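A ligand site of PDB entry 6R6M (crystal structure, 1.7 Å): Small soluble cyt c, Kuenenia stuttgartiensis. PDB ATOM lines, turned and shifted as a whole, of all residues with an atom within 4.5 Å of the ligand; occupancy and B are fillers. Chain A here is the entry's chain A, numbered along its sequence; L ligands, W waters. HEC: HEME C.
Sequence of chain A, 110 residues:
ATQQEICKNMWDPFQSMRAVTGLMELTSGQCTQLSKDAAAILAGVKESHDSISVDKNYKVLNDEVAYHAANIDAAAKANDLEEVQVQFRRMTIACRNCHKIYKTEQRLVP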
ATOM      1  N   GLN A   3     -15.798  15.204  10.249  1.00  0.00           N
ATOM      2  CA  GLN A   3     -17.059  14.475  10.315  1.00  0.00           C
ATOM      3  C   GLN A   3     -16.870  13.047   9.822  1.00  0.00           C
ATOM      4  O   GLN A   3     -17.420  12.106  10.418  1.00  0.00           O
ATOM      5  CB  GLN A   3     -18.131  15.192   9.499  1.00  0.00           C
ATOM      6  CG  GLN A   3     -19.514  14.554   9.662  1.00  0.00           C
ATOM      7  CD  GLN A   3     -20.043  14.667  11.084  1.00  0.00           C
ATOM      8  OE1 GLN A   3     -20.106  15.769  11.641  1.00  0.00           O
ATOM      9  NE2 GLN A   3     -20.419  13.532  11.671  1.00  0.00           N
ATOM     10  N   GLN A   4     -16.087  12.849   8.755  1.00  0.00           N
ATOM     11  CA  GLN A   4     -15.905  11.500   8.228  1.00  0.00           C
ATOM     12  C   GLN A   4     -15.250  10.587   9.265  1.00  0.00           C
ATOM     13  O   GLN A   4     -15.616   9.409   9.380  1.00  0.00           O
ATOM     14  CB  GLN A   4     -15.051  11.550   6.950  1.00  0.00           C
ATOM     15  CG  GLN A   4     -14.880  10.203   6.276  1.00  0.00           C
ATOM     16  CD  GLN A   4     -14.007  10.280   5.060  1.00  0.00           C
ATOM     17  OE1 GLN A   4     -13.148  11.146   4.955  1.00  0.00           O
ATOM     18  NE2 GLN A   4     -14.224   9.380   4.107  1.00  0.00           N
ATOM     19  N   CYS A   7     -17.950   9.868  12.069  1.00  0.00           N
ATOM     20  CA  CYS A   7     -18.976   8.913  11.673  1.00  0.00           C
ATOM     21  C   CYS A   7     -18.417   7.513  11.481  1.00  0.00           C
ATOM     22  O   CYS A   7     -19.060   6.519  11.845  1.00  0.00           O
ATOM     23  CB  CYS A   7     -19.681   9.403  10.410  1.00  0.00           C
ATOM     24  SG  CYS A   7     -20.955  10.608  10.800  1.00  0.00           S
ATOM     25  N   LYS A   8     -17.209   7.409  10.895  1.00  0.00           N
ATOM     26  CA  LYS A   8     -16.550   6.103  10.772  1.00  0.00           C
ATOM     27  C   LYS A   8     -16.444   5.415  12.111  1.00  0.00           C
ATOM     28  O   LYS A   8     -16.640   4.199  12.207  1.00  0.00           O
ATOM     29  CB  LYS A   8     -15.156   6.265  10.174  1.00  0.00           C
ATOM     30  CG  LYS A   8     -15.087   6.179   8.660  1.00  0.00           C
ATOM     31  CD  LYS A   8     -13.705   5.763   8.175  1.00  0.00           C
ATOM     32  CE  LYS A   8     -13.288   6.581   6.957  1.00  0.00           C
ATOM     33  NZ  LYS A   8     -13.105   5.737   5.735  1.00  0.00           N
ATOM     34  N   MET A  10     -18.477   5.774  14.600  1.00  0.00           N
ATOM     35  CA  MET A  10     -19.804   5.392  15.076  1.00  0.00           C
ATOM     36  C   MET A  10     -20.359   4.176  14.343  1.00  0.00           C
ATOM     37  O   MET A  10     -21.380   3.637  14.778  1.00  0.00           O
ATOM     38  CB  MET A  10     -20.806   6.543  14.912  1.00  0.00           C
ATOM     39  CG  MET A  10     -20.544   7.782  15.792  1.00  0.00           C
ATOM     40  SD  MET A  10     -21.966   8.900  15.921  1.00  0.00           S
ATOM     41  CE  MET A  10     -22.065   9.551  14.249  1.00  0.00           C
ATOM     42  N   TRP A  11     -19.730   3.737  13.246  1.00  0.00           N
ATOM     43  CA  TRP A  11     -20.370   2.752  12.383  1.00  0.00           C
ATOM     44  C   TRP A  11     -20.409   1.371  13.031  1.00  0.00           C
ATOM     45  O   TRP A  11     -21.424   0.678  12.962  1.00  0.00           O
ATOM     46  CB  TRP A  11     -19.658   2.694  11.029  1.00  0.00           C
ATOM     47  CG  TRP A  11     -20.299   1.720  10.088  1.00  0.00           C
ATOM     48  CD1 TRP A  11     -19.707   0.644   9.497  1.00  0.00           C
ATOM     49  CD2 TRP A  11     -21.659   1.717   9.639  1.00  0.00           C
ATOM     50  NE1 TRP A  11     -20.597  -0.028   8.715  1.00  0.00           N
ATOM     51  CE2 TRP A  11     -21.816   0.615   8.788  1.00  0.00           C
ATOM     52  CE3 TRP A  11     -22.772   2.545   9.880  1.00  0.00           C
ATOM     53  CZ2 TRP A  11     -23.023   0.314   8.156  1.00  0.00           C
ATOM     54  CZ3 TRP A  11     -23.974   2.233   9.268  1.00  0.00           C
ATOM     55  CH2 TRP A  11     -24.089   1.129   8.419  1.00  0.00           C
ATOM     56  N   PHE A  14     -23.009   1.422  15.748  1.00  0.00           N
ATOM     57  CA  PHE A  14     -24.319   1.401  15.094  1.00  0.00           C
ATOM     58  C   PHE A  14     -24.680  -0.013  14.646  1.00  0.00           C
ATOM     59  O   PHE A  14     -25.806  -0.469  14.847  1.00  0.00           O
ATOM     60  CB  PHE A  14     -24.329   2.371  13.910  1.00  0.00           C
ATOM     61  CG  PHE A  14     -25.630   2.377  13.154  1.00  0.00           C
ATOM     62  CD1 PHE A  14     -26.676   3.207  13.539  1.00  0.00           C
ATOM     63  CD2 PHE A  14     -25.811   1.541  12.054  1.00  0.00           C
ATOM     64  CE1 PHE A  14     -27.882   3.215  12.842  1.00  0.00           C
ATOM     65  CE2 PHE A  14     -27.025   1.537  11.358  1.00  0.00           C
ATOM     66  CZ  PHE A  14     -28.064   2.372  11.749  1.00  0.00           C
ATOM     67  N   ILE A  41     -22.343   6.442  20.217  1.00  0.00           N
ATOM     68  CA  ILE A  41     -23.043   7.317  19.281  1.00  0.00           C
ATOM     69  C   ILE A  41     -23.289   8.676  19.914  1.00  0.00           C
ATOM     70  O   ILE A  41     -23.063   9.721  19.283  1.00  0.00           O
ATOM     71  CB  ILE A  41     -24.340   6.638  18.806  1.00  0.00           C
ATOM     72  CG1 ILE A  41     -23.960   5.493  17.861  1.00  0.00           C
ATOM     73  CG2 ILE A  41     -25.264   7.628  18.127  1.00  0.00           C
ATOM     74  CD1 ILE A  41     -25.049   4.499  17.606  1.00  0.00           C
ATOM     75  N   SER A  48     -19.333  15.994  17.073  1.00  0.00           N
ATOM     76  CA  SER A  48     -19.688  16.714  15.853  1.00  0.00           C
ATOM     77  C   SER A  48     -20.318  18.056  16.195  1.00  0.00           C
ATOM     78  O   SER A  48     -19.923  19.100  15.674  1.00  0.00           O
ATOM     79  CB  SER A  48     -20.647  15.876  15.002  1.00  0.00           C
ATOM     80  OG  SER A  48     -21.084  16.617  13.868  1.00  0.00           O
ATOM     81  N   TYR A  58     -27.174  21.912  11.588  1.00  0.00           N
ATOM     82  CA  TYR A  58     -26.224  20.839  11.843  1.00  0.00           C
ATOM     83  C   TYR A  58     -26.195  20.473  13.326  1.00  0.00           C
ATOM     84  O   TYR A  58     -26.088  19.291  13.676  1.00  0.00           O
ATOM     85  CB  TYR A  58     -24.838  21.285  11.386  1.00  0.00           C
ATOM     86  CG  TYR A  58     -23.897  20.189  10.966  1.00  0.00           C
ATOM     87  CD1 TYR A  58     -24.025  19.592   9.703  1.00  0.00           C
ATOM     88  CD2 TYR A  58     -22.882  19.742  11.800  1.00  0.00           C
ATOM     89  CE1 TYR A  58     -23.157  18.607   9.304  1.00  0.00           C
ATOM     90  CE2 TYR A  58     -22.001  18.748  11.408  1.00  0.00           C
ATOM     91  CZ  TYR A  58     -22.162  18.182  10.144  1.00  0.00           C
ATOM     92  OH  TYR A  58     -21.285  17.213   9.720  1.00  0.00           O
ATOM     93  N   LEU A  61     -29.526  18.615  14.144  1.00  0.00           N
ATOM     94  CA  LEU A  61     -29.505  17.268  13.583  1.00  0.00           C
ATOM     95  C   LEU A  61     -28.707  16.314  14.477  1.00  0.00           C
ATOM     96  O   LEU A  61     -29.124  15.184  14.740  1.00  0.00           O
ATOM     97  CB  LEU A  61     -28.926  17.293  12.168  1.00  0.00           C
ATOM     98  CG  LEU A  61     -29.861  17.879  11.111  1.00  0.00           C
ATOM     99  CD1 LEU A  61     -29.064  18.422   9.943  1.00  0.00           C
ATOM    100  CD2 LEU A  61     -30.886  16.847  10.632  1.00  0.00           C
ATOM    101  N   ASN A  62     -27.536  16.770  14.945  1.00  0.00           N
ATOM    102  CA  ASN A  62     -26.807  15.992  15.946  1.00  0.00           C
ATOM    103  C   ASN A  62     -27.662  15.767  17.183  1.00  0.00           C
ATOM    104  O   ASN A  62     -27.713  14.648  17.713  1.00  0.00           O
ATOM    105  CB  ASN A  62     -25.501  16.705  16.311  1.00  0.00           C
ATOM    106  CG  ASN A  62     -24.357  16.370  15.350  1.00  0.00           C
ATOM    107  OD1 ASN A  62     -24.046  15.193  15.129  1.00  0.00           O
ATOM    108  ND2 ASN A  62     -23.747  17.392  14.776  1.00  0.00           N
ATOM    109  N   VAL A  65     -30.177  12.892  16.721  1.00  0.00           N
ATOM    110  CA  VAL A  65     -29.597  11.564  16.888  1.00  0.00           C
ATOM    111  C   VAL A  65     -29.408  11.262  18.372  1.00  0.00           C
ATOM    112  O   VAL A  65     -29.730  10.173  18.840  1.00  0.00           O
ATOM    113  CB  VAL A  65     -28.255  11.456  16.125  1.00  0.00           C
ATOM    114  CG1 VAL A  65     -27.579  10.118  16.428  1.00  0.00           C
ATOM    115  CG2 VAL A  65     -28.478  11.644  14.631  1.00  0.00           C
ATOM    116  N   MET A  91     -33.687   6.669  15.417  1.00  0.00           N
ATOM    117  CA  MET A  91     -32.308   7.151  15.381  1.00  0.00           C
ATOM    118  C   MET A  91     -31.713   6.988  13.988  1.00  0.00           C
ATOM    119  O   MET A  91     -30.957   7.839  13.528  1.00  0.00           O
ATOM    120  CB  MET A  91     -31.451   6.410  16.408  1.00  0.00           C
ATOM    121  CG  MET A  91     -30.047   7.025  16.519  1.00  0.00           C
ATOM    122  SD  MET A  91     -28.961   6.026  17.520  1.00  0.00           S
ATOM    123  CE  MET A  91     -28.508   4.703  16.393  1.00  0.00           C
ATOM    124  N   ALA A  94     -32.681   9.749  11.947  1.00  0.00           N
ATOM    125  CA  ALA A  94     -31.940  10.938  12.351  1.00  0.00           C
ATOM    126  C   ALA A  94     -30.558  10.977  11.722  1.00  0.00           C
ATOM    127  O   ALA A  94     -30.109  12.042  11.260  1.00  0.00           O
ATOM    128  CB  ALA A  94     -31.848  10.995  13.885  1.00  0.00           C
ATOM    129  N   CYS A  95     -29.853   9.838  11.696  1.00  0.00           N
ATOM    130  CA  CYS A  95     -28.591   9.761  10.970  1.00  0.00           C
ATOM    131  C   CYS A  95     -28.784  10.136   9.504  1.00  0.00           C
ATOM    132  O   CYS A  95     -28.080  10.988   8.965  1.00  0.00           O
ATOM    133  CB  CYS A  95     -27.995   8.354  11.055  1.00  0.00           C
ATOM    134  SG  CYS A  95     -27.719   7.657  12.686  1.00  0.00           S
ATOM    135  N   CYS A  98     -29.273  13.965   8.352  1.00  0.00           N
ATOM    136  CA  CYS A  98     -28.088  14.789   8.128  1.00  0.00           C
ATOM    137  C   CYS A  98     -27.418  14.430   6.813  1.00  0.00           C
ATOM    138  O   CYS A  98     -27.015  15.317   6.051  1.00  0.00           O
ATOM    139  CB  CYS A  98     -27.092  14.659   9.284  1.00  0.00           C
ATOM    140  SG  CYS A  98     -25.739  15.850   9.079  1.00  0.00           S
ATOM    141  N   HIS A  99     -27.314  13.129   6.519  1.00  0.00           N
ATOM    142  CA  HIS A  99     -26.660  12.695   5.283  1.00  0.00           C
ATOM    143  C   HIS A  99     -27.386  13.253   4.063  1.00  0.00           C
ATOM    144  O   HIS A  99     -26.751  13.728   3.110  1.00  0.00           O
ATOM    145  CB  HIS A  99     -26.593  11.176   5.222  1.00  0.00           C
ATOM    146  CG  HIS A  99     -25.715  10.576   6.271  1.00  0.00           C
ATOM    147  ND1 HIS A  99     -25.691   9.229   6.551  1.00  0.00           N
ATOM    148  CD2 HIS A  99     -24.834  11.159   7.118  1.00  0.00           C
ATOM    149  CE1 HIS A  99     -24.829   9.000   7.525  1.00  0.00           C
ATOM    150  NE2 HIS A  99     -24.285  10.155   7.881  1.00  0.00           N
ATOM    151  N   LYS A 103     -24.810  15.826   2.748  1.00  0.00           N
ATOM    152  CA  LYS A 103     -24.046  15.099   1.728  1.00  0.00           C
ATOM    153  C   LYS A 103     -24.996  14.544   0.681  1.00  0.00           C
ATOM    154  O   LYS A 103     -24.978  13.350   0.373  1.00  0.00           O
ATOM    155  CB  LYS A 103     -23.217  13.988   2.355  1.00  0.00           C
ATOM    156  CG  LYS A 103     -22.030  14.496   3.132  1.00  0.00           C
ATOM    157  CD  LYS A 103     -20.983  15.181   2.252  1.00  0.00           C
ATOM    158  CE  LYS A 103     -20.219  14.188   1.404  1.00  0.00           C
ATOM    159  NZ  LYS A 103     -19.100  14.819   0.654  1.00  0.00           N
ATOM    160  N   GLN A 106     -24.035  12.046  -2.319  1.00  0.00           N
ATOM    161  CA  GLN A 106     -23.227  10.857  -2.046  1.00  0.00           C
ATOM    162  C   GLN A 106     -24.108   9.774  -1.410  1.00  0.00           C
ATOM    163  O   GLN A 106     -24.842  10.048  -0.461  1.00  0.00           O
ATOM    164  CB  GLN A 106     -22.061  11.180  -1.116  1.00  0.00           C
ATOM    165  CG  GLN A 106     -21.045  10.047  -1.035  1.00  0.00           C
ATOM    166  CD  GLN A 106     -20.249  10.072   0.262  1.00  0.00           C
ATOM    167  OE1 GLN A 106     -19.856  11.126   0.756  1.00  0.00           O
ATOM    168  NE2 GLN A 106     -19.994   8.887   0.820  1.00  0.00           N
ATOM    169  N   LEU A 108     -24.852   7.177   1.065  1.00  0.00           N
ATOM    170  CA  LEU A 108     -24.357   6.973   2.415  1.00  0.00           C
ATOM    171  C   LEU A 108     -25.226   5.968   3.151  1.00  0.00           C
ATOM    172  O   LEU A 108     -26.422   5.812   2.868  1.00  0.00           O
ATOM    173  CB  LEU A 108     -24.290   8.274   3.204  1.00  0.00           C
ATOM    174  CG  LEU A 108     -23.032   9.117   2.965  1.00  0.00           C
ATOM    175  CD1 LEU A 108     -23.148  10.508   3.590  1.00  0.00           C
ATOM    176  CD2 LEU A 108     -21.843   8.363   3.507  1.00  0.00           C
ATOM    177  N   VAL A 109     -24.616   5.283   4.102  1.00  0.00           N
ATOM    178  CA  VAL A 109     -25.328   4.440   5.048  1.00  0.00           C
ATOM    179  C   VAL A 109     -25.602   5.303   6.278  1.00  0.00           C
ATOM    180  O   VAL A 109     -24.875   6.281   6.512  1.00  0.00           O
ATOM    181  CB  VAL A 109     -24.524   3.185   5.412  1.00  0.00           C
ATOM    182  CG1 VAL A 109     -24.342   2.315   4.176  1.00  0.00           C
ATOM    183  CG2 VAL A 109     -23.165   3.575   5.982  1.00  0.00           C
ATOM    184  N   PRO A 110     -26.642   5.007   7.075  1.00  0.00           N
ATOM    185  CA  PRO A 110     -27.610   3.918   6.941  1.00  0.00           C
ATOM    186  C   PRO A 110     -28.851   4.289   6.127  1.00  0.00           C
ATOM    187  O   PRO A 110     -29.701   3.447   5.832  1.00  0.00           O
ATOM    188  CB  PRO A 110     -27.993   3.620   8.382  1.00  0.00           C
ATOM    189  CG  PRO A 110     -27.937   4.959   9.049  1.00  0.00           C
ATOM    190  CD  PRO A 110     -26.892   5.786   8.307  1.00  0.00           C
ATOM    191  OXT PRO A 110     -29.050   5.454   5.762  1.00  0.00           O
HETATM  192 FE   HEC L   1     -22.777  10.371   9.197  1.00  0.00          FE
HETATM  193  CHA HEC L   1     -20.526  10.067   6.575  1.00  0.00           C
HETATM  194  CHB HEC L   1     -22.722   7.012   9.633  1.00  0.00           C
HETATM  195  CHC HEC L   1     -25.040  10.678  11.778  1.00  0.00           C
HETATM  196  CHD HEC L   1     -22.894  13.770   8.753  1.00  0.00           C
HETATM  197  NA  HEC L   1     -21.841   8.876   8.230  1.00  0.00           N
HETATM  198  C1A HEC L   1     -20.873   8.929   7.252  1.00  0.00           C
HETATM  199  C2A HEC L   1     -20.309   7.612   7.060  1.00  0.00           C
HETATM  200  C3A HEC L   1     -20.928   6.775   7.906  1.00  0.00           C
HETATM  201  C4A HEC L   1     -21.898   7.547   8.666  1.00  0.00           C
HETATM  202  CMA HEC L   1     -20.648   5.261   8.056  1.00  0.00           C
HETATM  203  CAA HEC L   1     -19.213   7.243   6.042  1.00  0.00           C
HETATM  204  CBA HEC L   1     -17.838   7.263   6.688  1.00  0.00           C
HETATM  205  CGA HEC L   1     -16.802   6.832   5.669  1.00  0.00           C
HETATM  206  O1A HEC L   1     -16.293   5.682   5.784  1.00  0.00           O
HETATM  207  O2A HEC L   1     -16.478   7.620   4.747  1.00  0.00           O
HETATM  208  NB  HEC L   1     -23.704   9.073  10.496  1.00  0.00           N
HETATM  209  C1B HEC L   1     -23.567   7.708  10.476  1.00  0.00           C
HETATM  210  C2B HEC L   1     -24.411   7.168  11.523  1.00  0.00           C
HETATM  211  C3B HEC L   1     -25.070   8.194  12.111  1.00  0.00           C
HETATM  212  C4B HEC L   1     -24.621   9.403  11.466  1.00  0.00           C
HETATM  213  CMB HEC L   1     -24.581   5.662  11.813  1.00  0.00           C
HETATM  214  CAB HEC L   1     -26.132   8.183  13.242  1.00  0.00           C
HETATM  215  CBB HEC L   1     -25.707   7.386  14.505  1.00  0.00           C
HETATM  216  NC  HEC L   1     -23.757  11.897  10.105  1.00  0.00           N
HETATM  217  C1C HEC L   1     -24.646  11.832  11.154  1.00  0.00           C
HETATM  218  C2C HEC L   1     -25.058  13.176  11.527  1.00  0.00           C
HETATM  219  C3C HEC L   1     -24.500  14.033  10.651  1.00  0.00           C
HETATM  220  C4C HEC L   1     -23.664  13.246   9.768  1.00  0.00           C
HETATM  221  CMC HEC L   1     -26.124  13.421  12.623  1.00  0.00           C
HETATM  222  CAC HEC L   1     -24.662  15.567  10.466  1.00  0.00           C
HETATM  223  CBC HEC L   1     -24.921  16.382  11.750  1.00  0.00           C
HETATM  224  ND  HEC L   1     -21.862  11.700   7.888  1.00  0.00           N
HETATM  225  C1D HEC L   1     -22.090  13.073   7.890  1.00  0.00           C
HETATM  226  C2D HEC L   1     -21.313  13.665   6.830  1.00  0.00           C
HETATM  227  C3D HEC L   1     -20.584  12.508   6.154  1.00  0.00           C
HETATM  228  C4D HEC L   1     -20.979  11.329   6.869  1.00  0.00           C
HETATM  229  CMD HEC L   1     -21.266  15.162   6.470  1.00  0.00           C
HETATM  230  CAD HEC L   1     -19.615  12.565   4.959  1.00  0.00           C
HETATM  231  CBD HEC L   1     -18.207  12.574   5.538  1.00  0.00           C
HETATM  232  CGD HEC L   1     -17.243  12.908   4.433  1.00  0.00           C
HETATM  233  O1D HEC L   1     -16.816  11.982   3.700  1.00  0.00           O
HETATM  234  O2D HEC L   1     -16.917  14.113   4.312  1.00  0.00           O
HETATM  235  O   HOH W   1     -22.599  13.420  13.754  1.00  0.00           O
HETATM  236  O   HOH W   2     -17.914   9.707   3.644  1.00  0.00           O
HETATM  237  O   HOH W   3     -15.496  15.054   6.914  1.00  0.00           O
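Merely in contact with the ligand: Gln 3, Met 10, Trp 11, Phe 14, Ile 41, Tyr 58, Asn 62, Val 65, Lys 103, Leu 108 and Val 109. The nearest printed residue that does not touch the ligand is Leu 61 (4.1 Å).
A ring nitrogen (ND1) of His 99 sits close to the backbone carbonyl oxygen (O) of Val 109, at 3.1 Å. OE1 of Gln 3 lies within hydrogen-bond range of OH of Tyr 58 (2.7 Å). The side-chain sulfur (SG) of Cys 7 lies close to the side-chain amide nitrogen (NE2) of Gln 3, 3.1 Å away. The side-chain amide nitrogen of Asn 62 is in hydrogen-bond range of the side-chain hydroxyl of Ser 48, 2.9 Å away. The backbone carbonyl oxygen (O) of Tyr 58 lies within hydrogen-bond range of the side-chain amide nitrogen (ND2) of Asn 62 (3.2 Å). OG of Ser 48 lies within hydrogen-bond range of OE1 of Gln 3.
SG of Cys 98 is covalently linked to CAC of the ligand (1.8 Å). NE2 of His 99 is bound to FE of the ligand, 2.0 Å away. A carbon (CAB) of the ligand is covalently linked to the side-chain sulfur (SG) of Cys 95, 1.8 Å away. An oxygen (O1A) of the ligand lies within salt-bridge range of the side-chain amino group (NZ) of Lys 8, at 3.2 Å. The side-chain sulfur (SG) of Cys 7 binds an iron atom (FE) of the ligand, 2.4 Å away. The side-chain amide nitrogen (NE2) of Gln 4 sits at hydrogen-bond distance from an oxygen (O2A) of the ligand (2.9 Å).
Water W3 lies within hydrogen-bond range of N of Gln 4 (2.9 Å), O2D of the ligand (3.1 Å) and N of Gln 3 (3.4 Å). Water W1 lies within hydrogen-bond range of OD1 of Asn 62 (2.7 Å) and NE2 of Gln 3 (3.0 Å).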
